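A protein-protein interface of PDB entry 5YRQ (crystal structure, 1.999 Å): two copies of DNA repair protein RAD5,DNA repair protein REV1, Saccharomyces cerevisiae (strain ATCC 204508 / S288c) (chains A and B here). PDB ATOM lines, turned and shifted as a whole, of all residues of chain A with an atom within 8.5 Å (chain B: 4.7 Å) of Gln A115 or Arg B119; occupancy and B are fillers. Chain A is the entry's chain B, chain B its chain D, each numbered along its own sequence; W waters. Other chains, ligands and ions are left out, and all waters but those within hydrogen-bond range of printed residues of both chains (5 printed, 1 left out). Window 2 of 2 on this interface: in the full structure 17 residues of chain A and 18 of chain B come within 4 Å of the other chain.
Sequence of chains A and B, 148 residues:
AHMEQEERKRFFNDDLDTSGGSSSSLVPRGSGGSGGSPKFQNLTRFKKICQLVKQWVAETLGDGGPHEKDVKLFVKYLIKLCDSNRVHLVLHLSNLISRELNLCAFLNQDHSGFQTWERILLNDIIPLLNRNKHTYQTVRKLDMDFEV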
ATOM      1  N   LEU A  61     -22.214  30.845  26.132  1.00  0.00           N
ATOM      2  CA  LEU A  61     -23.531  30.890  25.499  1.00  0.00           C
ATOM      3  C   LEU A  61     -23.468  31.594  24.149  1.00  0.00           C
ATOM      4  O   LEU A  61     -23.983  31.085  23.145  1.00  0.00           O
ATOM      5  CB  LEU A  61     -24.544  31.581  26.418  1.00  0.00           C
ATOM      6  CG  LEU A  61     -25.179  30.644  27.447  1.00  0.00           C
ATOM      7  CD1 LEU A  61     -25.788  31.413  28.607  1.00  0.00           C
ATOM      8  CD2 LEU A  61     -26.220  29.769  26.775  1.00  0.00           C
ATOM      9  N   GLY A  64     -22.227  29.556  21.006  1.00  0.00           N
ATOM     10  CA  GLY A  64     -22.862  28.308  20.657  1.00  0.00           C
ATOM     11  C   GLY A  64     -22.601  27.168  21.621  1.00  0.00           C
ATOM     12  O   GLY A  64     -23.073  26.053  21.377  1.00  0.00           O
ATOM     13  N   GLY A  65     -21.876  27.409  22.708  1.00  0.00           N
ATOM     14  CA  GLY A  65     -21.662  26.394  23.704  1.00  0.00           C
ATOM     15  C   GLY A  65     -20.222  26.339  24.163  1.00  0.00           C
ATOM     16  O   GLY A  65     -19.351  27.039  23.642  1.00  0.00           O
ATOM     17  N   PRO A  66     -19.948  25.508  25.157  1.00  0.00           N
ATOM     18  CA  PRO A  66     -18.601  25.418  25.712  1.00  0.00           C
ATOM     19  C   PRO A  66     -17.779  24.349  25.006  1.00  0.00           C
ATOM     20  O   PRO A  66     -18.292  23.542  24.234  1.00  0.00           O
ATOM     21  CB  PRO A  66     -18.866  25.031  27.168  1.00  0.00           C
ATOM     22  CG  PRO A  66     -20.077  24.184  27.086  1.00  0.00           C
ATOM     23  CD  PRO A  66     -20.907  24.707  25.932  1.00  0.00           C
ATOM     24  N   LEU A 101     -29.367  30.086  31.987  1.00  0.00           N
ATOM     25  CA  LEU A 101     -30.127  29.845  30.765  1.00  0.00           C
ATOM     26  C   LEU A 101     -31.441  30.629  30.737  1.00  0.00           C
ATOM     27  O   LEU A 101     -31.984  30.862  29.654  1.00  0.00           O
ATOM     28  CB  LEU A 101     -30.382  28.350  30.597  1.00  0.00           C
ATOM     29  CG  LEU A 101     -29.156  27.428  30.512  1.00  0.00           C
ATOM     30  CD1 LEU A 101     -29.546  26.007  30.140  1.00  0.00           C
ATOM     31  CD2 LEU A 101     -28.090  27.948  29.555  1.00  0.00           C
ATOM     32  N   CYS A 104     -30.971  33.813  28.719  1.00  0.00           N
ATOM     33  CA  CYS A 104     -31.177  33.572  27.289  1.00  0.00           C
ATOM     34  C   CYS A 104     -32.653  33.530  26.940  1.00  0.00           C
ATOM     35  O   CYS A 104     -33.099  34.178  25.984  1.00  0.00           O
ATOM     36  CB  CYS A 104     -30.555  32.243  26.851  1.00  0.00           C
ATOM     37  SG  CYS A 104     -28.885  32.030  27.263  1.00  0.00           S
ATOM     38  N   GLN A 109     -32.276  35.096  23.014  1.00  0.00           N
ATOM     39  CA  GLN A 109     -30.973  35.253  22.395  1.00  0.00           C
ATOM     40  C   GLN A 109     -30.201  33.956  22.568  1.00  0.00           C
ATOM     41  O   GLN A 109     -30.540  33.124  23.411  1.00  0.00           O
ATOM     42  CB  GLN A 109     -30.189  36.421  23.015  1.00  0.00           C
ATOM     43  CG  GLN A 109     -29.793  36.196  24.471  1.00  0.00           C
ATOM     44  CD  GLN A 109     -29.186  37.434  25.121  1.00  0.00           C
ATOM     45  OE1 GLN A 109     -29.509  38.563  24.751  1.00  0.00           O
ATOM     46  NE2 GLN A 109     -28.304  37.222  26.091  1.00  0.00           N
ATOM     47  N   ASP A 110     -29.177  33.784  21.732  1.00  0.00           N
ATOM     48  CA  ASP A 110     -28.172  32.735  21.910  1.00  0.00           C
ATOM     49  C   ASP A 110     -28.782  31.334  21.857  1.00  0.00           C
ATOM     50  O   ASP A 110     -28.441  30.469  22.671  1.00  0.00           O
ATOM     51  CB  ASP A 110     -27.409  32.926  23.226  1.00  0.00           C
ATOM     52  CG  ASP A 110     -26.509  34.148  23.213  1.00  0.00           C
ATOM     53  OD1 ASP A 110     -26.045  34.539  22.126  1.00  0.00           O
ATOM     54  OD2 ASP A 110     -26.260  34.714  24.298  1.00  0.00           O
ATOM     55  N   HIS A 111     -29.674  31.095  20.879  1.00  0.00           N
ATOM     56  CA  HIS A 111     -30.445  29.852  20.885  1.00  0.00           C
ATOM     57  C   HIS A 111     -29.550  28.630  20.724  1.00  0.00           C
ATOM     58  O   HIS A 111     -29.841  27.574  21.303  1.00  0.00           O
ATOM     59  CB  HIS A 111     -31.520  29.875  19.793  1.00  0.00           C
ATOM     60  CG  HIS A 111     -32.539  30.960  19.971  1.00  0.00           C
ATOM     61  ND1 HIS A 111     -32.254  32.288  19.746  1.00  0.00           N
ATOM     62  CD2 HIS A 111     -33.838  30.913  20.350  1.00  0.00           C
ATOM     63  CE1 HIS A 111     -33.332  33.014  19.981  1.00  0.00           C
ATOM     64  NE2 HIS A 111     -34.308  32.203  20.351  1.00  0.00           N
ATOM     65  N   SER A 112     -28.453  28.755  19.968  1.00  0.00           N
ATOM     66  CA  SER A 112     -27.546  27.624  19.782  1.00  0.00           C
ATOM     67  C   SER A 112     -26.829  27.260  21.082  1.00  0.00           C
ATOM     68  O   SER A 112     -26.798  26.087  21.484  1.00  0.00           O
ATOM     69  CB  SER A 112     -26.537  27.953  18.682  1.00  0.00           C
ATOM     70  OG  SER A 112     -25.635  26.880  18.483  1.00  0.00           O
ATOM     71  N   GLY A 113     -26.241  28.256  21.753  1.00  0.00           N
ATOM     72  CA  GLY A 113     -25.561  27.999  23.012  1.00  0.00           C
ATOM     73  C   GLY A 113     -26.503  27.558  24.109  1.00  0.00           C
ATOM     74  O   GLY A 113     -26.129  26.740  24.958  1.00  0.00           O
ATOM     75  N   PHE A 114     -27.728  28.101  24.124  1.00  0.00           N
ATOM     76  CA  PHE A 114     -28.745  27.605  25.047  1.00  0.00           C
ATOM     77  C   PHE A 114     -28.950  26.106  24.874  1.00  0.00           C
ATOM     78  O   PHE A 114     -28.916  25.344  25.849  1.00  0.00           O
ATOM     79  CB  PHE A 114     -30.082  28.323  24.842  1.00  0.00           C
ATOM     80  CG  PHE A 114     -31.182  27.762  25.707  1.00  0.00           C
ATOM     81  CD1 PHE A 114     -31.447  28.314  26.951  1.00  0.00           C
ATOM     82  CD2 PHE A 114     -31.907  26.650  25.315  1.00  0.00           C
ATOM     83  CE1 PHE A 114     -32.433  27.783  27.770  1.00  0.00           C
ATOM     84  CE2 PHE A 114     -32.889  26.105  26.142  1.00  0.00           C
ATOM     85  CZ  PHE A 114     -33.141  26.676  27.379  1.00  0.00           C
ATOM     86  N   GLN A 115     -29.199  25.668  23.637  1.00  0.00           N
ATOM     87  CA  GLN A 115     -29.523  24.263  23.411  1.00  0.00           C
ATOM     88  C   GLN A 115     -28.357  23.362  23.778  1.00  0.00           C
ATOM     89  O   GLN A 115     -28.556  22.277  24.337  1.00  0.00           O
ATOM     90  CB  GLN A 115     -29.947  24.055  21.962  1.00  0.00           C
ATOM     91  CG  GLN A 115     -31.291  24.701  21.668  1.00  0.00           C
ATOM     92  CD  GLN A 115     -31.708  24.537  20.242  1.00  0.00           C
ATOM     93  OE1 GLN A 115     -31.162  23.701  19.529  1.00  0.00           O
ATOM     94  NE2 GLN A 115     -32.682  25.338  19.807  1.00  0.00           N
ATOM     95  N   THR A 116     -27.134  23.797  23.487  1.00  0.00           N
ATOM     96  CA  THR A 116     -25.975  22.996  23.856  1.00  0.00           C
ATOM     97  C   THR A 116     -25.811  22.945  25.368  1.00  0.00           C
ATOM     98  O   THR A 116     -25.608  21.865  25.949  1.00  0.00           O
ATOM     99  CB  THR A 116     -24.721  23.547  23.178  1.00  0.00           C
ATOM    100  OG1 THR A 116     -24.860  23.410  21.753  1.00  0.00           O
ATOM    101  CG2 THR A 116     -23.478  22.782  23.647  1.00  0.00           C
ATOM    102  N   TRP A 117     -25.925  24.103  26.034  1.00  0.00           N
ATOM    103  CA  TRP A 117     -25.833  24.122  27.491  1.00  0.00           C
ATOM    104  C   TRP A 117     -26.983  23.367  28.131  1.00  0.00           C
ATOM    105  O   TRP A 117     -26.805  22.740  29.188  1.00  0.00           O
ATOM    106  CB  TRP A 117     -25.801  25.559  28.027  1.00  0.00           C
ATOM    107  CG  TRP A 117     -24.412  26.037  28.246  1.00  0.00           C
ATOM    108  CD1 TRP A 117     -23.754  27.007  27.541  1.00  0.00           C
ATOM    109  CD2 TRP A 117     -23.486  25.546  29.218  1.00  0.00           C
ATOM    110  NE1 TRP A 117     -22.475  27.157  28.029  1.00  0.00           N
ATOM    111  CE2 TRP A 117     -22.285  26.264  29.051  1.00  0.00           C
ATOM    112  CE3 TRP A 117     -23.554  24.565  30.214  1.00  0.00           C
ATOM    113  CZ2 TRP A 117     -21.169  26.048  29.857  1.00  0.00           C
ATOM    114  CZ3 TRP A 117     -22.443  24.349  31.008  1.00  0.00           C
ATOM    115  CH2 TRP A 117     -21.264  25.087  30.826  1.00  0.00           C
ATOM    116  N   GLU A 118     -28.163  23.430  27.513  1.00  0.00           N
ATOM    117  CA  GLU A 118     -29.326  22.756  28.067  1.00  0.00           C
ATOM    118  C   GLU A 118     -29.120  21.253  28.057  1.00  0.00           C
ATOM    119  O   GLU A 118     -29.432  20.571  29.042  1.00  0.00           O
ATOM    120  CB  GLU A 118     -30.582  23.151  27.278  1.00  0.00           C
ATOM    121  CG  GLU A 118     -31.877  22.531  27.770  1.00  0.00           C
ATOM    122  CD  GLU A 118     -33.033  22.808  26.837  1.00  0.00           C
ATOM    123  OE1 GLU A 118     -34.096  23.260  27.317  1.00  0.00           O
ATOM    124  OE2 GLU A 118     -32.875  22.579  25.616  1.00  0.00           O
ATOM    125  N   ARG A 119     -28.589  20.720  26.947  1.00  0.00           N
ATOM    126  CA  ARG A 119     -28.307  19.290  26.865  1.00  0.00           C
ATOM    127  C   ARG A 119     -27.292  18.874  27.918  1.00  0.00           C
ATOM    128  O   ARG A 119     -27.450  17.840  28.577  1.00  0.00           O
ATOM    129  CB  ARG A 119     -27.804  18.922  25.463  1.00  0.00           C
ATOM    130  CG  ARG A 119     -27.122  17.549  25.436  1.00  0.00           C
ATOM    131  CD  ARG A 119     -26.740  17.051  24.046  1.00  0.00           C
ATOM    132  NE  ARG A 119     -25.782  17.909  23.356  1.00  0.00           N
ATOM    133  CZ  ARG A 119     -24.488  17.992  23.645  1.00  0.00           C
ATOM    134  NH1 ARG A 119     -23.974  17.277  24.636  1.00  0.00           N
ATOM    135  NH2 ARG A 119     -23.707  18.803  22.945  1.00  0.00           N
ATOM    136  N   ILE A 120     -26.249  19.683  28.107  1.00  0.00           N
ATOM    137  CA  ILE A 120     -25.261  19.404  29.142  1.00  0.00           C
ATOM    138  C   ILE A 120     -25.926  19.358  30.514  1.00  0.00           C
ATOM    139  O   ILE A 120     -25.688  18.442  31.312  1.00  0.00           O
ATOM    140  CB  ILE A 120     -24.134  20.451  29.085  1.00  0.00           C
ATOM    141  CG1 ILE A 120     -23.324  20.277  27.797  1.00  0.00           C
ATOM    142  CG2 ILE A 120     -23.236  20.335  30.310  1.00  0.00           C
ATOM    143  CD1 ILE A 120     -22.446  21.470  27.462  1.00  0.00           C
ATOM    144  N   LEU A 121     -26.785  20.339  30.801  1.00  0.00           N
ATOM    145  CA  LEU A 121     -27.496  20.365  32.078  1.00  0.00           C
ATOM    146  C   LEU A 121     -28.361  19.119  32.259  1.00  0.00           C
ATOM    147  O   LEU A 121     -28.291  18.442  33.292  1.00  0.00           O
ATOM    148  CB  LEU A 121     -28.352  21.636  32.177  1.00  0.00           C
ATOM    149  CG  LEU A 121     -29.116  21.804  33.498  1.00  0.00           C
ATOM    150  CD1 LEU A 121     -28.193  22.122  34.700  1.00  0.00           C
ATOM    151  CD2 LEU A 121     -30.197  22.848  33.387  1.00  0.00           C
ATOM    152  N   LEU A 122     -29.173  18.793  31.253  1.00  0.00           N
ATOM    153  CA  LEU A 122     -30.158  17.728  31.384  1.00  0.00           C
ATOM    154  C   LEU A 122     -29.541  16.332  31.254  1.00  0.00           C
ATOM    155  O   LEU A 122     -30.030  15.382  31.880  1.00  0.00           O
ATOM    156  CB  LEU A 122     -31.264  17.920  30.335  1.00  0.00           C
ATOM    157  CG  LEU A 122     -32.110  19.211  30.342  1.00  0.00           C
ATOM    158  CD1 LEU A 122     -32.958  19.315  29.079  1.00  0.00           C
ATOM    159  CD2 LEU A 122     -33.006  19.299  31.577  1.00  0.00           C
ATOM    160  N   ASN A 123     -28.482  16.174  30.456  1.00  0.00           N
ATOM    161  CA  ASN A 123     -27.924  14.852  30.186  1.00  0.00           C
ATOM    162  C   ASN A 123     -26.618  14.555  30.903  1.00  0.00           C
ATOM    163  O   ASN A 123     -26.345  13.382  31.205  1.00  0.00           O
ATOM    164  CB  ASN A 123     -27.688  14.667  28.683  1.00  0.00           C
ATOM    165  CG  ASN A 123     -28.972  14.610  27.892  1.00  0.00           C
ATOM    166  OD1 ASN A 123     -28.972  14.885  26.697  1.00  0.00           O
ATOM    167  ND2 ASN A 123     -30.075  14.256  28.552  1.00  0.00           N
ATOM    168  N   GLN B 115     -26.040  11.133  22.052  1.00  0.00           N
ATOM    169  CA  GLN B 115     -26.743  12.269  22.643  1.00  0.00           C
ATOM    170  C   GLN B 115     -26.528  13.536  21.834  1.00  0.00           C
ATOM    171  O   GLN B 115     -27.468  14.304  21.618  1.00  0.00           O
ATOM    172  CB  GLN B 115     -26.303  12.461  24.091  1.00  0.00           C
ATOM    173  CG  GLN B 115     -26.796  11.341  24.995  1.00  0.00           C
ATOM    174  CD  GLN B 115     -26.332  11.485  26.419  1.00  0.00           C
ATOM    175  OE1 GLN B 115     -25.867  12.551  26.825  1.00  0.00           O
ATOM    176  NE2 GLN B 115     -26.450  10.406  27.194  1.00  0.00           N
ATOM    177  N   THR B 116     -25.310  13.759  21.350  1.00  0.00           N
ATOM    178  CA  THR B 116     -25.066  14.931  20.512  1.00  0.00           C
ATOM    179  C   THR B 116     -25.829  14.841  19.191  1.00  0.00           C
ATOM    180  O   THR B 116     -26.487  15.806  18.772  1.00  0.00           O
ATOM    181  CB  THR B 116     -23.567  15.088  20.265  1.00  0.00           C
ATOM    182  OG1 THR B 116     -22.921  15.410  21.500  1.00  0.00           O
ATOM    183  CG2 THR B 116     -23.305  16.203  19.247  1.00  0.00           C
ATOM    184  N   TRP B 117     -25.757  13.682  18.515  1.00  0.00           N
ATOM    185  CA  TRP B 117     -26.489  13.513  17.257  1.00  0.00           C
ATOM    186  C   TRP B 117     -27.987  13.569  17.487  1.00  0.00           C
ATOM    187  O   TRP B 117     -28.744  14.051  16.632  1.00  0.00           O
ATOM    188  CB  TRP B 117     -26.127  12.182  16.571  1.00  0.00           C
ATOM    189  CG  TRP B 117     -25.052  12.323  15.522  1.00  0.00           C
ATOM    190  CD1 TRP B 117     -23.792  11.782  15.558  1.00  0.00           C
ATOM    191  CD2 TRP B 117     -25.136  13.066  14.299  1.00  0.00           C
ATOM    192  NE1 TRP B 117     -23.090  12.145  14.428  1.00  0.00           N
ATOM    193  CE2 TRP B 117     -23.890  12.937  13.644  1.00  0.00           C
ATOM    194  CE3 TRP B 117     -26.141  13.828  13.694  1.00  0.00           C
ATOM    195  CZ2 TRP B 117     -23.630  13.528  12.407  1.00  0.00           C
ATOM    196  CZ3 TRP B 117     -25.875  14.429  12.468  1.00  0.00           C
ATOM    197  CH2 TRP B 117     -24.632  14.274  11.835  1.00  0.00           C
ATOM    198  N   GLU B 118     -28.440  13.029  18.613  1.00  0.00           N
ATOM    199  CA  GLU B 118     -29.869  13.062  18.902  1.00  0.00           C
ATOM    200  C   GLU B 118     -30.360  14.497  19.008  1.00  0.00           C
ATOM    201  O   GLU B 118     -31.423  14.842  18.464  1.00  0.00           O
ATOM    202  CB  GLU B 118     -30.156  12.281  20.185  1.00  0.00           C
ATOM    203  CG  GLU B 118     -31.615  12.258  20.622  1.00  0.00           C
ATOM    204  CD  GLU B 118     -31.788  11.569  21.961  1.00  0.00           C
ATOM    205  OE1 GLU B 118     -31.075  11.940  22.919  1.00  0.00           O
ATOM    206  OE2 GLU B 118     -32.614  10.641  22.053  1.00  0.00           O
ATOM    207  N   ARG B 119     -29.577  15.351  19.676  1.00  0.00           N
ATOM    208  CA  ARG B 119     -29.928  16.759  19.824  1.00  0.00           C
ATOM    209  C   ARG B 119     -29.953  17.457  18.470  1.00  0.00           C
ATOM    210  O   ARG B 119     -30.846  18.272  18.197  1.00  0.00           O
ATOM    211  CB  ARG B 119     -28.940  17.454  20.774  1.00  0.00           C
ATOM    212  CG  ARG B 119     -29.154  18.973  20.864  1.00  0.00           C
ATOM    213  CD  ARG B 119     -28.104  19.718  21.697  1.00  0.00           C
ATOM    214  NE  ARG B 119     -26.726  19.457  21.285  1.00  0.00           N
ATOM    215  CZ  ARG B 119     -26.047  20.171  20.393  1.00  0.00           C
ATOM    216  NH1 ARG B 119     -26.616  21.207  19.792  1.00  0.00           N
ATOM    217  NH2 ARG B 119     -24.798  19.840  20.097  1.00  0.00           N
ATOM    218  N   ILE B 120     -28.983  17.142  17.611  1.00  0.00           N
ATOM    219  CA  ILE B 120     -28.979  17.680  16.256  1.00  0.00           C
ATOM    220  C   ILE B 120     -30.235  17.244  15.513  1.00  0.00           C
ATOM    221  O   ILE B 120     -30.908  18.054  14.867  1.00  0.00           O
ATOM    222  CB  ILE B 120     -27.699  17.245  15.521  1.00  0.00           C
ATOM    223  CG1 ILE B 120     -26.485  17.919  16.161  1.00  0.00           C
ATOM    224  CG2 ILE B 120     -27.804  17.530  14.012  1.00  0.00           C
ATOM    225  CD1 ILE B 120     -25.180  17.276  15.779  1.00  0.00           C
ATOM    226  N   LEU B 121     -30.573  15.958  15.602  1.00  0.00           N
ATOM    227  CA  LEU B 121     -31.771  15.455  14.933  1.00  0.00           C
ATOM    228  C   LEU B 121     -33.025  16.174  15.423  1.00  0.00           C
ATOM    229  O   LEU B 121     -33.852  16.635  14.622  1.00  0.00           O
ATOM    230  CB  LEU B 121     -31.899  13.947  15.162  1.00  0.00           C
ATOM    231  CG  LEU B 121     -33.154  13.308  14.557  1.00  0.00           C
ATOM    232  CD1 LEU B 121     -33.134  13.365  13.014  1.00  0.00           C
ATOM    233  CD2 LEU B 121     -33.328  11.879  15.043  1.00  0.00           C
ATOM    234  N   LEU B 122     -33.182  16.282  16.742  1.00  0.00           N
ATOM    235  CA  LEU B 122     -34.445  16.751  17.296  1.00  0.00           C
ATOM    236  C   LEU B 122     -34.563  18.270  17.285  1.00  0.00           C
ATOM    237  O   LEU B 122     -35.673  18.798  17.162  1.00  0.00           O
ATOM    238  CB  LEU B 122     -34.619  16.230  18.723  1.00  0.00           C
ATOM    239  CG  LEU B 122     -34.664  14.720  18.962  1.00  0.00           C
ATOM    240  CD1 LEU B 122     -34.559  14.424  20.455  1.00  0.00           C
ATOM    241  CD2 LEU B 122     -35.928  14.089  18.367  1.00  0.00           C
ATOM    242  N   ASN B 123     -33.451  18.992  17.414  1.00  0.00           N
ATOM    243  CA  ASN B 123     -33.522  20.446  17.535  1.00  0.00           C
ATOM    244  C   ASN B 123     -33.100  21.202  16.283  1.00  0.00           C
ATOM    245  O   ASN B 123     -33.562  22.334  16.072  1.00  0.00           O
ATOM    246  CB  ASN B 123     -32.658  20.907  18.708  1.00  0.00           C
ATOM    247  CG  ASN B 123     -33.203  20.452  20.047  1.00  0.00           C
ATOM    248  OD1 ASN B 123     -34.384  20.113  20.177  1.00  0.00           O
ATOM    249  ND2 ASN B 123     -32.343  20.460  21.061  1.00  0.00           N
ATOM    250  N   ASP B 124     -32.223  20.628  15.456  1.00  0.00           N
ATOM    251  CA  ASP B 124     -31.721  21.322  14.273  1.00  0.00           C
ATOM    252  C   ASP B 124     -32.337  20.820  12.980  1.00  0.00           C
ATOM    253  O   ASP B 124     -32.508  21.605  12.043  1.00  0.00           O
ATOM    254  CB  ASP B 124     -30.195  21.183  14.168  1.00  0.00           C
ATOM    255  CG  ASP B 124     -29.477  21.721  15.391  1.00  0.00           C
ATOM    256  OD1 ASP B 124     -28.714  20.962  16.020  1.00  0.00           O
ATOM    257  OD2 ASP B 124     -29.669  22.907  15.720  1.00  0.00           O
HETATM  258  O   HOH W   1     -24.529  14.997  26.245  1.00  0.00           O
HETATM  259  O   HOH W   2     -22.332  14.935  24.716  1.00  0.00           O
HETATM  260  O   HOH W   3     -34.734  24.036  17.684  1.00  0.00           O
HETATM  261  O   HOH W   4     -27.499  10.952  30.226  1.00  0.00           O
HETATM  262  O   HOH W   5     -26.879  23.806  19.084  1.00  0.00           O
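The guanidinium group of Arg A119 lies close to the guanidinium group of Arg B119 (2.8 Å). OG1 of Thr A116 is in hydrogen-bond range of NH1 of Arg B119.
The backbone carbonyl oxygen of Ser A112 lies within hydrogen-bond range of the side-chain hydroxyl of Thr A116, at 3.3 Å. O of Gly A64 lies within hydrogen-bond range of OG1 of Thr A116 (3.2 Å).
Among the printed residues, pairs that only touch across the chains: Gln A115 with Asn B123 (3.3 Å), Asn A123 with Gln B115 (3.4 Å), Gln A115 with Arg B119 (3.7 Å), Arg A119 with Thr B116 (3.7 Å) and Arg A119 with Gln B115 (3.7 Å).
Gln A115 touches just these residues of chain B: Arg B119 (3.7 Å) and Asn B123 (3.3 Å). Printed residues of chain B within 4 Å of Thr A116: Arg B119 (3.4 Å). Printed residues of chain B within 4 Å of Arg A119: Gln B115, Thr B116 and Arg B119. Printed residues of chain B within 4 Å of Asn A123: Gln B115 (3.4 Å). Of the printed residues of chain A, Gln B115 touches Arg A119 (3.7 Å) and Asn A123 (3.4 Å). Printed residues of chain A within 4 Å of Arg B119: Gln A115, Thr A116 and Arg A119. Of the printed residues of chain A, Asn B123 touches Gln A115. Asp B124 touches none of the printed residues of chain A. The nearest residue of chain A that does not touch Arg B119 is Ser A112 (5.2 Å). The nearest printed residue of chain B that does not touch Thr A116 is Asn B123 (6.6 Å).
Printed residues of chain A that touch a printed residue of chain B: Gln A115, Thr A116, Arg A119 and Asn A123. Among the printed residues, 7 pairs touch across the chains.
Gln A115 touches Arg B119, and with the chains exchanged Arg A119 touches Gln B115. Gln A115 touches Asn B123, and with the chains exchanged Asn A123 touches Gln B115. Thr A116 touches Arg B119, and with the chains exchanged Arg A119 touches Thr B116. Arg A119 touches its own counterpart, Arg B119. Positions printed for both chains: 115, 116, 117, 118, 119, 120, 121, 122 and 123. Of the 7 pairs that touch across the chains among the printed residues, 7 have their exchanged pair printed and touching as well.
Water W3 lies within hydrogen-bond range of the backbone carbonyl oxygen (O) of Asn B123 (2.6 Å) and the side-chain amide nitrogen (NE2) of Gln A115 (3.2 Å). Water W5 lies within hydrogen-bond range of the guanidinium group of Arg B119 (2.7 Å), the backbone carbonyl oxygen of Ser A112 (3.3 Å) and the side-chain hydroxyl of Thr A116 (3.4 Å). Water W1 lies within hydrogen-bond range of NH1 of Arg A119 (2.8 Å) and OE1 of Gln B115 (2.8 Å). Water W2 lies within hydrogen-bond range of the guanidinium group (NH1) of Arg A119 (2.9 Å) and the side-chain hydroxyl (OG1) of Thr B116 (3.3 Å). Water W4 bridges the backbone carbonyl oxygen (O) of Asn A123 and the side-chain amide nitrogen (NE2) of Gln B115.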
